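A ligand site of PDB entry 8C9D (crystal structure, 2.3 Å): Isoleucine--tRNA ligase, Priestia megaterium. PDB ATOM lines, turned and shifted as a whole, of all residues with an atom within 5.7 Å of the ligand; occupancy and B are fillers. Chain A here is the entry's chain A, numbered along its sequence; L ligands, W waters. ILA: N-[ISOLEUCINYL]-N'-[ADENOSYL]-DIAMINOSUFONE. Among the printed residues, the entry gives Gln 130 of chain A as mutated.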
ATOM      1  N   GLY A  45       7.113 -21.473 -12.032  1.00  0.00           N
ATOM      2  CA  GLY A  45       7.791 -21.957 -13.206  1.00  0.00           C
ATOM      3  C   GLY A  45       6.950 -21.678 -14.447  1.00  0.00           C
ATOM      4  O   GLY A  45       5.784 -22.084 -14.521  1.00  0.00           O
ATOM      5  N   PRO A  46       7.523 -20.982 -15.425  1.00  0.00           N
ATOM      6  CA  PRO A  46       6.715 -20.518 -16.566  1.00  0.00           C
ATOM      7  C   PRO A  46       6.465 -21.636 -17.570  1.00  0.00           C
ATOM      8  O   PRO A  46       7.412 -22.134 -18.198  1.00  0.00           O
ATOM      9  CB  PRO A  46       7.593 -19.404 -17.175  1.00  0.00           C
ATOM     10  CG  PRO A  46       9.001 -19.830 -16.854  1.00  0.00           C
ATOM     11  CD  PRO A  46       8.932 -20.591 -15.532  1.00  0.00           C
ATOM     12  N   PRO A  47       5.213 -22.034 -17.761  1.00  0.00           N
ATOM     13  CA  PRO A  47       4.911 -23.061 -18.767  1.00  0.00           C
ATOM     14  C   PRO A  47       5.242 -22.565 -20.165  1.00  0.00           C
ATOM     15  O   PRO A  47       5.099 -21.385 -20.475  1.00  0.00           O
ATOM     16  CB  PRO A  47       3.403 -23.299 -18.608  1.00  0.00           C
ATOM     17  CG  PRO A  47       3.081 -22.768 -17.227  1.00  0.00           C
ATOM     18  CD  PRO A  47       4.002 -21.600 -17.049  1.00  0.00           C
ATOM     19  N   THR A  48       5.705 -23.484 -21.018  1.00  0.00           N
ATOM     20  CA  THR A  48       5.980 -23.151 -22.403  1.00  0.00           C
ATOM     21  C   THR A  48       4.680 -22.915 -23.160  1.00  0.00           C
ATOM     22  O   THR A  48       3.732 -23.698 -23.029  1.00  0.00           O
ATOM     23  CB  THR A  48       6.769 -24.283 -23.070  1.00  0.00           C
ATOM     24  OG1 THR A  48       7.946 -24.576 -22.311  1.00  0.00           O
ATOM     25  CG2 THR A  48       7.195 -23.893 -24.484  1.00  0.00           C
ATOM     26  N   HIS A  54      -2.201 -30.846 -20.885  1.00  0.00           N
ATOM     27  CA  HIS A  54      -2.756 -32.168 -20.644  1.00  0.00           C
ATOM     28  C   HIS A  54      -2.825 -32.397 -19.138  1.00  0.00           C
ATOM     29  O   HIS A  54      -2.394 -31.562 -18.338  1.00  0.00           O
ATOM     30  CB  HIS A  54      -1.951 -33.255 -21.376  1.00  0.00           C
ATOM     31  CG  HIS A  54      -0.527 -33.361 -20.946  1.00  0.00           C
ATOM     32  ND1 HIS A  54      -0.143 -33.420 -19.621  1.00  0.00           N
ATOM     33  CD2 HIS A  54       0.615 -33.438 -21.673  1.00  0.00           C
ATOM     34  CE1 HIS A  54       1.172 -33.521 -19.553  1.00  0.00           C
ATOM     35  NE2 HIS A  54       1.659 -33.529 -20.775  1.00  0.00           N
ATOM     36  N   GLY A  56      -1.295 -34.115 -17.028  1.00  0.00           N
ATOM     37  CA  GLY A  56      -0.044 -34.024 -16.274  1.00  0.00           C
ATOM     38  C   GLY A  56       0.242 -32.614 -15.796  1.00  0.00           C
ATOM     39  O   GLY A  56       0.667 -32.412 -14.646  1.00  0.00           O
ATOM     40  N   HIS A  57      -0.027 -31.619 -16.635  1.00  0.00           N
ATOM     41  CA  HIS A  57       0.206 -30.231 -16.267  1.00  0.00           C
ATOM     42  C   HIS A  57      -0.705 -29.752 -15.155  1.00  0.00           C
ATOM     43  O   HIS A  57      -0.469 -28.674 -14.602  1.00  0.00           O
ATOM     44  CB  HIS A  57       0.054 -29.327 -17.485  1.00  0.00           C
ATOM     45  CG  HIS A  57       0.956 -29.681 -18.615  1.00  0.00           C
ATOM     46  ND1 HIS A  57       0.499 -30.002 -19.875  1.00  0.00           N
ATOM     47  CD2 HIS A  57       2.312 -29.782 -18.687  1.00  0.00           C
ATOM     48  CE1 HIS A  57       1.523 -30.282 -20.666  1.00  0.00           C
ATOM     49  NE2 HIS A  57       2.626 -30.157 -19.962  1.00  0.00           N
ATOM     50  N   LEU A  59      -0.910 -31.410 -12.346  1.00  0.00           N
ATOM     51  CA  LEU A  59      -0.314 -31.831 -11.082  1.00  0.00           C
ATOM     52  C   LEU A  59       0.400 -30.678 -10.387  1.00  0.00           C
ATOM     53  O   LEU A  59       0.028 -30.272  -9.278  1.00  0.00           O
ATOM     54  CB  LEU A  59       0.632 -33.015 -11.304  1.00  0.00           C
ATOM     55  CG  LEU A  59       1.280 -33.600 -10.042  1.00  0.00           C
ATOM     56  CD1 LEU A  59       0.246 -34.007  -9.002  1.00  0.00           C
ATOM     57  CD2 LEU A  59       2.182 -34.790 -10.399  1.00  0.00           C
ATOM     58  N   GLY A  60       1.413 -30.115 -11.053  1.00  0.00           N
ATOM     59  CA  GLY A  60       2.173 -29.031 -10.429  1.00  0.00           C
ATOM     60  C   GLY A  60       1.293 -27.859 -10.051  1.00  0.00           C
ATOM     61  O   GLY A  60       1.339 -27.377  -8.913  1.00  0.00           O
ATOM     62  N   ARG A  61       0.452 -27.411 -10.987  1.00  0.00           N
ATOM     63  CA  ARG A  61      -0.470 -26.311 -10.697  1.00  0.00           C
ATOM     64  C   ARG A  61      -1.279 -26.608  -9.445  1.00  0.00           C
ATOM     65  O   ARG A  61      -1.483 -25.727  -8.604  1.00  0.00           O
ATOM     66  CB  ARG A  61      -1.407 -26.075 -11.884  1.00  0.00           C
ATOM     67  CG  ARG A  61      -0.728 -25.607 -13.154  1.00  0.00           C
ATOM     68  CD  ARG A  61      -1.711 -25.683 -14.313  1.00  0.00           C
ATOM     69  NE  ARG A  61      -1.469 -24.698 -15.354  1.00  0.00           N
ATOM     70  CZ  ARG A  61      -0.747 -24.921 -16.444  1.00  0.00           C
ATOM     71  NH1 ARG A  61      -0.129 -26.083 -16.626  1.00  0.00           N
ATOM     72  NH2 ARG A  61      -0.649 -23.983 -17.366  1.00  0.00           N
ATOM     73  N   ASP A  85       6.733 -19.015 -20.792  1.00  0.00           N
ATOM     74  CA  ASP A  85       7.993 -19.270 -21.497  1.00  0.00           C
ATOM     75  C   ASP A  85       7.713 -19.259 -22.993  1.00  0.00           C
ATOM     76  O   ASP A  85       7.021 -20.138 -23.508  1.00  0.00           O
ATOM     77  CB  ASP A  85       8.548 -20.634 -21.065  1.00  0.00           C
ATOM     78  CG  ASP A  85      10.058 -20.676 -21.022  1.00  0.00           C
ATOM     79  OD1 ASP A  85      10.598 -21.696 -20.537  1.00  0.00           O
ATOM     80  OD2 ASP A  85      10.710 -19.705 -21.460  1.00  0.00           O
ATOM     81  N   GLN A 130      -3.626 -21.891 -21.984  1.00  0.00           N
ATOM     82  CA  GLN A 130      -3.069 -22.228 -20.674  1.00  0.00           C
ATOM     83  C   GLN A 130      -3.757 -21.434 -19.558  1.00  0.00           C
ATOM     84  O   GLN A 130      -4.049 -21.991 -18.489  1.00  0.00           O
ATOM     85  CB  GLN A 130      -1.560 -21.965 -20.655  1.00  0.00           C
ATOM     86  CG  GLN A 130      -0.783 -22.771 -21.679  1.00  0.00           C
ATOM     87  CD  GLN A 130       0.028 -23.890 -21.046  1.00  0.00           C
ATOM     88  OE1 GLN A 130       0.090 -24.011 -19.819  1.00  0.00           O
ATOM     89  NE2 GLN A 130       0.647 -24.714 -21.881  1.00  0.00           N
ATOM     90  N   TRP A 517      16.529 -22.091 -21.704  1.00  0.00           N
ATOM     91  CA  TRP A 517      16.667 -22.358 -20.273  1.00  0.00           C
ATOM     92  C   TRP A 517      17.274 -21.172 -19.546  1.00  0.00           C
ATOM     93  O   TRP A 517      16.965 -20.959 -18.369  1.00  0.00           O
ATOM     94  CB  TRP A 517      17.490 -23.626 -20.048  1.00  0.00           C
ATOM     95  CG  TRP A 517      16.749 -24.859 -20.453  1.00  0.00           C
ATOM     96  CD1 TRP A 517      17.048 -25.704 -21.469  1.00  0.00           C
ATOM     97  CD2 TRP A 517      15.548 -25.358 -19.857  1.00  0.00           C
ATOM     98  NE1 TRP A 517      16.130 -26.707 -21.544  1.00  0.00           N
ATOM     99  CE2 TRP A 517      15.193 -26.523 -20.565  1.00  0.00           C
ATOM    100  CE3 TRP A 517      14.737 -24.935 -18.792  1.00  0.00           C
ATOM    101  CZ2 TRP A 517      14.050 -27.275 -20.243  1.00  0.00           C
ATOM    102  CZ3 TRP A 517      13.610 -25.687 -18.476  1.00  0.00           C
ATOM    103  CH2 TRP A 517      13.281 -26.843 -19.195  1.00  0.00           C
ATOM    104  N   SER A 520      14.317 -18.828 -18.700  1.00  0.00           N
ATOM    105  CA  SER A 520      13.520 -19.214 -17.529  1.00  0.00           C
ATOM    106  C   SER A 520      14.341 -19.148 -16.248  1.00  0.00           C
ATOM    107  O   SER A 520      13.810 -18.789 -15.190  1.00  0.00           O
ATOM    108  CB  SER A 520      12.922 -20.614 -17.720  1.00  0.00           C
ATOM    109  OG  SER A 520      13.946 -21.588 -17.899  1.00  0.00           O
ATOM    110  N   ALA A 548       7.925 -25.769  -7.100  1.00  0.00           N
ATOM    111  CA  ALA A 548       7.342 -27.101  -7.285  1.00  0.00           C
ATOM    112  C   ALA A 548       7.075 -27.319  -8.773  1.00  0.00           C
ATOM    113  O   ALA A 548       6.185 -26.670  -9.343  1.00  0.00           O
ATOM    114  CB  ALA A 548       6.059 -27.257  -6.469  1.00  0.00           C
ATOM    115  N   GLU A 549       7.849 -28.205  -9.393  1.00  0.00           N
ATOM    116  CA  GLU A 549       7.721 -28.520 -10.807  1.00  0.00           C
ATOM    117  C   GLU A 549       8.095 -29.980 -11.014  1.00  0.00           C
ATOM    118  O   GLU A 549       8.535 -30.671 -10.087  1.00  0.00           O
ATOM    119  CB  GLU A 549       8.589 -27.618 -11.688  1.00  0.00           C
ATOM    120  CG  GLU A 549       8.383 -26.123 -11.480  1.00  0.00           C
ATOM    121  CD  GLU A 549       7.049 -25.619 -11.996  1.00  0.00           C
ATOM    122  OE1 GLU A 549       6.482 -26.252 -12.917  1.00  0.00           O
ATOM    123  OE2 GLU A 549       6.553 -24.601 -11.454  1.00  0.00           O
ATOM    124  N   GLY A 550       7.954 -30.449 -12.257  1.00  0.00           N
ATOM    125  CA  GLY A 550       8.213 -31.840 -12.557  1.00  0.00           C
ATOM    126  C   GLY A 550       9.690 -32.195 -12.529  1.00  0.00           C
ATOM    127  O   GLY A 550      10.578 -31.342 -12.652  1.00  0.00           O
ATOM    128  N   ILE A 551       9.950 -33.500 -12.392  1.00  0.00           N
ATOM    129  CA  ILE A 551      11.294 -34.019 -12.212  1.00  0.00           C
ATOM    130  C   ILE A 551      12.197 -33.699 -13.387  1.00  0.00           C
ATOM    131  O   ILE A 551      13.427 -33.638 -13.233  1.00  0.00           O
ATOM    132  CB  ILE A 551      11.246 -35.546 -11.938  1.00  0.00           C
ATOM    133  CG1 ILE A 551      12.612 -36.070 -11.483  1.00  0.00           C
ATOM    134  CG2 ILE A 551      10.763 -36.302 -13.171  1.00  0.00           C
ATOM    135  CD1 ILE A 551      12.590 -37.522 -11.053  1.00  0.00           C
ATOM    136  N   ASP A 552      11.634 -33.491 -14.581  1.00  0.00           N
ATOM    137  CA  ASP A 552      12.455 -33.168 -15.744  1.00  0.00           C
ATOM    138  C   ASP A 552      13.212 -31.858 -15.564  1.00  0.00           C
ATOM    139  O   ASP A 552      14.262 -31.671 -16.187  1.00  0.00           O
ATOM    140  CB  ASP A 552      11.590 -33.108 -17.005  1.00  0.00           C
ATOM    141  CG  ASP A 552      10.361 -32.236 -16.839  1.00  0.00           C
ATOM    142  OD1 ASP A 552       9.615 -32.427 -15.853  1.00  0.00           O
ATOM    143  OD2 ASP A 552      10.141 -31.351 -17.700  1.00  0.00           O
ATOM    144  N   GLN A 553      12.722 -30.972 -14.702  1.00  0.00           N
ATOM    145  CA  GLN A 553      13.428 -29.738 -14.437  1.00  0.00           C
ATOM    146  C   GLN A 553      14.763 -29.952 -13.716  1.00  0.00           C
ATOM    147  O   GLN A 553      15.550 -29.001 -13.628  1.00  0.00           O
ATOM    148  CB  GLN A 553      12.546 -28.783 -13.612  1.00  0.00           C
ATOM    149  CG  GLN A 553      11.135 -28.598 -14.172  1.00  0.00           C
ATOM    150  CD  GLN A 553      11.130 -28.139 -15.622  1.00  0.00           C
ATOM    151  OE1 GLN A 553      12.111 -27.590 -16.129  1.00  0.00           O
ATOM    152  NE2 GLN A 553       9.997 -28.344 -16.296  1.00  0.00           N
ATOM    153  N   TRP A 557      14.676 -26.299 -15.377  1.00  0.00           N
ATOM    154  CA  TRP A 557      14.517 -25.052 -14.653  1.00  0.00           C
ATOM    155  C   TRP A 557      15.234 -25.074 -13.311  1.00  0.00           C
ATOM    156  O   TRP A 557      15.750 -24.050 -12.865  1.00  0.00           O
ATOM    157  CB  TRP A 557      13.034 -24.747 -14.473  1.00  0.00           C
ATOM    158  CG  TRP A 557      12.740 -23.350 -14.005  1.00  0.00           C
ATOM    159  CD1 TRP A 557      13.181 -22.185 -14.579  1.00  0.00           C
ATOM    160  CD2 TRP A 557      11.916 -22.975 -12.899  1.00  0.00           C
ATOM    161  NE1 TRP A 557      12.683 -21.112 -13.877  1.00  0.00           N
ATOM    162  CE2 TRP A 557      11.905 -21.563 -12.841  1.00  0.00           C
ATOM    163  CE3 TRP A 557      11.187 -23.699 -11.949  1.00  0.00           C
ATOM    164  CZ2 TRP A 557      11.192 -20.857 -11.875  1.00  0.00           C
ATOM    165  CZ3 TRP A 557      10.487 -22.997 -10.981  1.00  0.00           C
ATOM    166  CH2 TRP A 557      10.487 -21.591 -10.959  1.00  0.00           C
ATOM    167  N   LEU A 580       8.329 -33.240  -8.812  1.00  0.00           N
ATOM    168  CA  LEU A 580       7.113 -34.028  -8.991  1.00  0.00           C
ATOM    169  C   LEU A 580       7.294 -35.076 -10.072  1.00  0.00           C
ATOM    170  O   LEU A 580       7.770 -34.773 -11.175  1.00  0.00           O
ATOM    171  CB  LEU A 580       5.932 -33.124  -9.336  1.00  0.00           C
ATOM    172  CG  LEU A 580       5.858 -31.893  -8.441  1.00  0.00           C
ATOM    173  CD1 LEU A 580       4.780 -30.936  -8.926  1.00  0.00           C
ATOM    174  CD2 LEU A 580       5.590 -32.315  -6.996  1.00  0.00           C
ATOM    175  N   GLY A 581       6.910 -36.311  -9.766  1.00  0.00           N
ATOM    176  CA  GLY A 581       6.883 -37.346 -10.774  1.00  0.00           C
ATOM    177  C   GLY A 581       5.847 -37.043 -11.838  1.00  0.00           C
ATOM    178  O   GLY A 581       4.817 -36.421 -11.582  1.00  0.00           O
ATOM    179  N   HIS A 582       6.137 -37.473 -13.068  1.00  0.00           N
ATOM    180  CA  HIS A 582       5.231 -37.223 -14.167  1.00  0.00           C
ATOM    181  C   HIS A 582       3.977 -38.075 -14.051  1.00  0.00           C
ATOM    182  O   HIS A 582       3.994 -39.169 -13.473  1.00  0.00           O
ATOM    183  CB  HIS A 582       5.923 -37.479 -15.508  1.00  0.00           C
ATOM    184  CG  HIS A 582       6.806 -36.356 -15.957  1.00  0.00           C
ATOM    185  ND1 HIS A 582       7.220 -36.210 -17.260  1.00  0.00           N
ATOM    186  CD2 HIS A 582       7.353 -35.323 -15.261  1.00  0.00           C
ATOM    187  CE1 HIS A 582       7.989 -35.133 -17.356  1.00  0.00           C
ATOM    188  NE2 HIS A 582       8.080 -34.582 -16.155  1.00  0.00           N
ATOM    189  N   VAL A 583       2.888 -37.572 -14.609  1.00  0.00           N
ATOM    190  CA  VAL A 583       1.631 -38.298 -14.720  1.00  0.00           C
ATOM    191  C   VAL A 583       1.659 -39.132 -15.991  1.00  0.00           C
ATOM    192  O   VAL A 583       1.983 -38.623 -17.077  1.00  0.00           O
ATOM    193  CB  VAL A 583       0.428 -37.343 -14.714  1.00  0.00           C
ATOM    194  CG1 VAL A 583      -0.855 -38.068 -15.092  1.00  0.00           C
ATOM    195  CG2 VAL A 583       0.278 -36.682 -13.350  1.00  0.00           C
ATOM    196  N   LYS A 590       3.736 -43.151 -21.053  1.00  0.00           N
ATOM    197  CA  LYS A 590       3.778 -41.691 -21.106  1.00  0.00           C
ATOM    198  C   LYS A 590       2.698 -41.182 -22.060  1.00  0.00           C
ATOM    199  O   LYS A 590       2.489 -41.727 -23.141  1.00  0.00           O
ATOM    200  CB  LYS A 590       5.163 -41.219 -21.566  1.00  0.00           C
ATOM    201  CG  LYS A 590       5.414 -39.716 -21.390  1.00  0.00           C
ATOM    202  CD  LYS A 590       4.829 -39.193 -20.082  1.00  0.00           C
ATOM    203  CE  LYS A 590       5.707 -38.111 -19.447  1.00  0.00           C
ATOM    204  NZ  LYS A 590       6.391 -37.248 -20.452  1.00  0.00           N
HETATM  205  N   ILA L   1       8.783 -23.916 -19.664  1.00  0.00           N
HETATM  206  CA  ILA L   1       9.502 -25.038 -19.086  1.00  0.00           C
HETATM  207  CB  ILA L   1       9.966 -24.803 -17.634  1.00  0.00           C
HETATM  208  CG2 ILA L   1      10.857 -23.566 -17.570  1.00  0.00           C
HETATM  209  CG1 ILA L   1       8.755 -24.670 -16.698  1.00  0.00           C
HETATM  210  CD  ILA L   1       9.102 -24.852 -15.226  1.00  0.00           C
HETATM  211  C   ILA L   1       8.571 -26.238 -19.153  1.00  0.00           C
HETATM  212  O   ILA L   1       8.943 -27.366 -18.921  1.00  0.00           O
HETATM  213  SA  ILA L   1       6.088 -27.147 -19.637  1.00  0.00           S
HETATM  214  O1A ILA L   1       4.863 -26.414 -19.852  1.00  0.00           O
HETATM  215  O2A ILA L   1       6.589 -28.105 -20.593  1.00  0.00           O
HETATM  216  N3A ILA L   1       7.276 -25.955 -19.494  1.00  0.00           N
HETATM  217  N5' ILA L   1       5.920 -27.916 -18.220  1.00  0.00           N
HETATM  218  C5' ILA L   1       5.079 -27.310 -17.206  1.00  0.00           C
HETATM  219  C4' ILA L   1       5.190 -28.128 -15.918  1.00  0.00           C
HETATM  220  O4' ILA L   1       4.572 -29.405 -16.108  1.00  0.00           O
HETATM  221  C1' ILA L   1       5.494 -30.433 -15.816  1.00  0.00           C
HETATM  222  N9  ILA L   1       5.196 -31.576 -16.625  1.00  0.00           N
HETATM  223  C4  ILA L   1       4.542 -32.699 -16.212  1.00  0.00           C
HETATM  224  N3  ILA L   1       4.057 -32.961 -14.994  1.00  0.00           N
HETATM  225  C2  ILA L   1       3.496 -34.156 -14.957  1.00  0.00           C
HETATM  226  N1  ILA L   1       3.365 -35.044 -15.940  1.00  0.00           N
HETATM  227  C6  ILA L   1       3.848 -34.762 -17.148  1.00  0.00           C
HETATM  228  N6  ILA L   1       3.721 -35.657 -18.134  1.00  0.00           N
HETATM  229  C5  ILA L   1       4.487 -33.518 -17.323  1.00  0.00           C
HETATM  230  N7  ILA L   1       5.079 -32.922 -18.409  1.00  0.00           N
HETATM  231  C8  ILA L   1       5.490 -31.783 -17.956  1.00  0.00           C
HETATM  232  C2' ILA L   1       6.875 -29.809 -16.041  1.00  0.00           C
HETATM  233  O2' ILA L   1       7.886 -30.510 -15.379  1.00  0.00           O
HETATM  234  C3' ILA L   1       6.625 -28.402 -15.482  1.00  0.00           C
HETATM  235  O3' ILA L   1       6.650 -28.449 -14.073  1.00  0.00           O
HETATM  236  O   HOH W   1       3.180 -26.401 -22.194  1.00  0.00           O
HETATM  237  O   HOH W   2       8.168 -30.198 -19.215  1.00  0.00           O
HETATM  238  O   HOH W   3       2.750 -30.627 -13.608  1.00  0.00           O
HETATM  239  O   HOH W   4       5.242 -30.855 -21.409  1.00  0.00           O
HETATM  240  O   HOH W   5       5.360 -24.733 -14.867  1.00  0.00           O
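OE1 of Glu 549 is in hydrogen-bond range of O3' of the ligand (2.5 Å).
An oxygen (O2') of the ligand lies within hydrogen-bond range of the side-chain carboxylate (OD1) of Asp 552.
A nitrogen (N) of the ligand is in hydrogen-bond range of the backbone carbonyl oxygen of Pro 46, 2.7 Å away.
O1A of the ligand sits at hydrogen-bond distance from N of Thr 48 (3.3 Å).
OG1 of Thr 48 lies within hydrogen-bond range of N of the ligand (2.9 Å).
The backbone NH (N) of Val 583 lies within hydrogen-bond range of a nitrogen (N1) of the ligand (2.9 Å).
NE2 of Gln 553 lies within hydrogen-bond range of O of the ligand, at 3.0 Å.
The side-chain carboxylate (OD1) of Asp 85 lies within salt-bridge range of a nitrogen (N) of the ligand (3.0 Å).
N of Gly 550 is in hydrogen-bond range of O3' of the ligand.
The side-chain carboxylate (OE2) of Glu 549 lies within hydrogen-bond range of the backbone NH (N) of Gly 45, at 3.2 Å.
The backbone NH of Leu 580 lies within hydrogen-bond range of the backbone carbonyl oxygen of Glu 549 (2.9 Å).
The side-chain amide oxygen (OE1) of Gln 553 lies within hydrogen-bond range of the backbone NH (N) of Trp 557 (3.0 Å).
O of Pro 47 is in hydrogen-bond range of N of Asp 85.
A ring nitrogen (ND1) of His 54 lies within hydrogen-bond range of the backbone NH (N) of Gly 56.
A ring nitrogen (ND1) of His 57 sits at hydrogen-bond distance from the backbone NH of His 54.
The guanidinium group (NH1) of Arg 61 lies close to the backbone carbonyl oxygen (O) of His 57, 3.3 Å away.
O of Trp 517 lies within hydrogen-bond range of OG of Ser 520 (3.1 Å).
Water W1 lies within hydrogen-bond range of O of Thr 48 (2.9 Å), O1A of the ligand (2.9 Å) and NE2 of Gln 130 (3.1 Å).
Water W2 lies within hydrogen-bond range of OD2 of Asp 552 (2.7 Å) and O of the ligand (3.0 Å).
Water W3 lies within hydrogen-bond range of the backbone NH of Gly 60 (2.9 Å), the backbone carbonyl oxygen of Gly 56 (2.9 Å) and a nitrogen (N3) of the ligand (3.0 Å).
Water W4 bridges a ring nitrogen (NE2) of His 57 (3.1 Å) and an oxygen (O2A) of the ligand (3.2 Å).
Water W5 lies within hydrogen-bond range of the backbone carbonyl oxygen of Gly 45 (2.7 Å) and the side-chain carboxylate of Glu 549 (2.7 Å).
The backbone carbonyl oxygen of Gly 56 lies close to a nitrogen (N3) of the ligand, 3.5 Å away.
Gly 45 touches the ligand.
CA of Pro 47 touches O1A of the ligand (3.5 Å).
His 54 touches the ligand (CE1 to N6, 3.6 Å).
His 57 touches the ligand (CD2 to O4', 3.4 Å).
Trp 517 touches the ligand.
Ser 520 touches the ligand.
Trp 557 touches the ligand (CB to CG2, 3.97 Å).
His 582 touches the ligand.
Lys 590 touches the ligand (CE to N6, 3.4 Å).
Hydrophobic or aromatic side chains within 4 Å of the ligand: Pro 47, His 54, His 57, Trp 517, Trp 557, His 582 and Val 583.
Within 4 Å of the ligand: Gly 45, Pro 46, Pro 47, Thr 48, His 54, Gly 56, His 57, Asp 85, Trp 517, Ser 520, Glu 549, Gly 550, Asp 552, Gln 553, Trp 557, His 582, Val 583 and Lys 590.
The nearest printed residue that does not touch the ligand is Gly 581 (4.3 Å).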
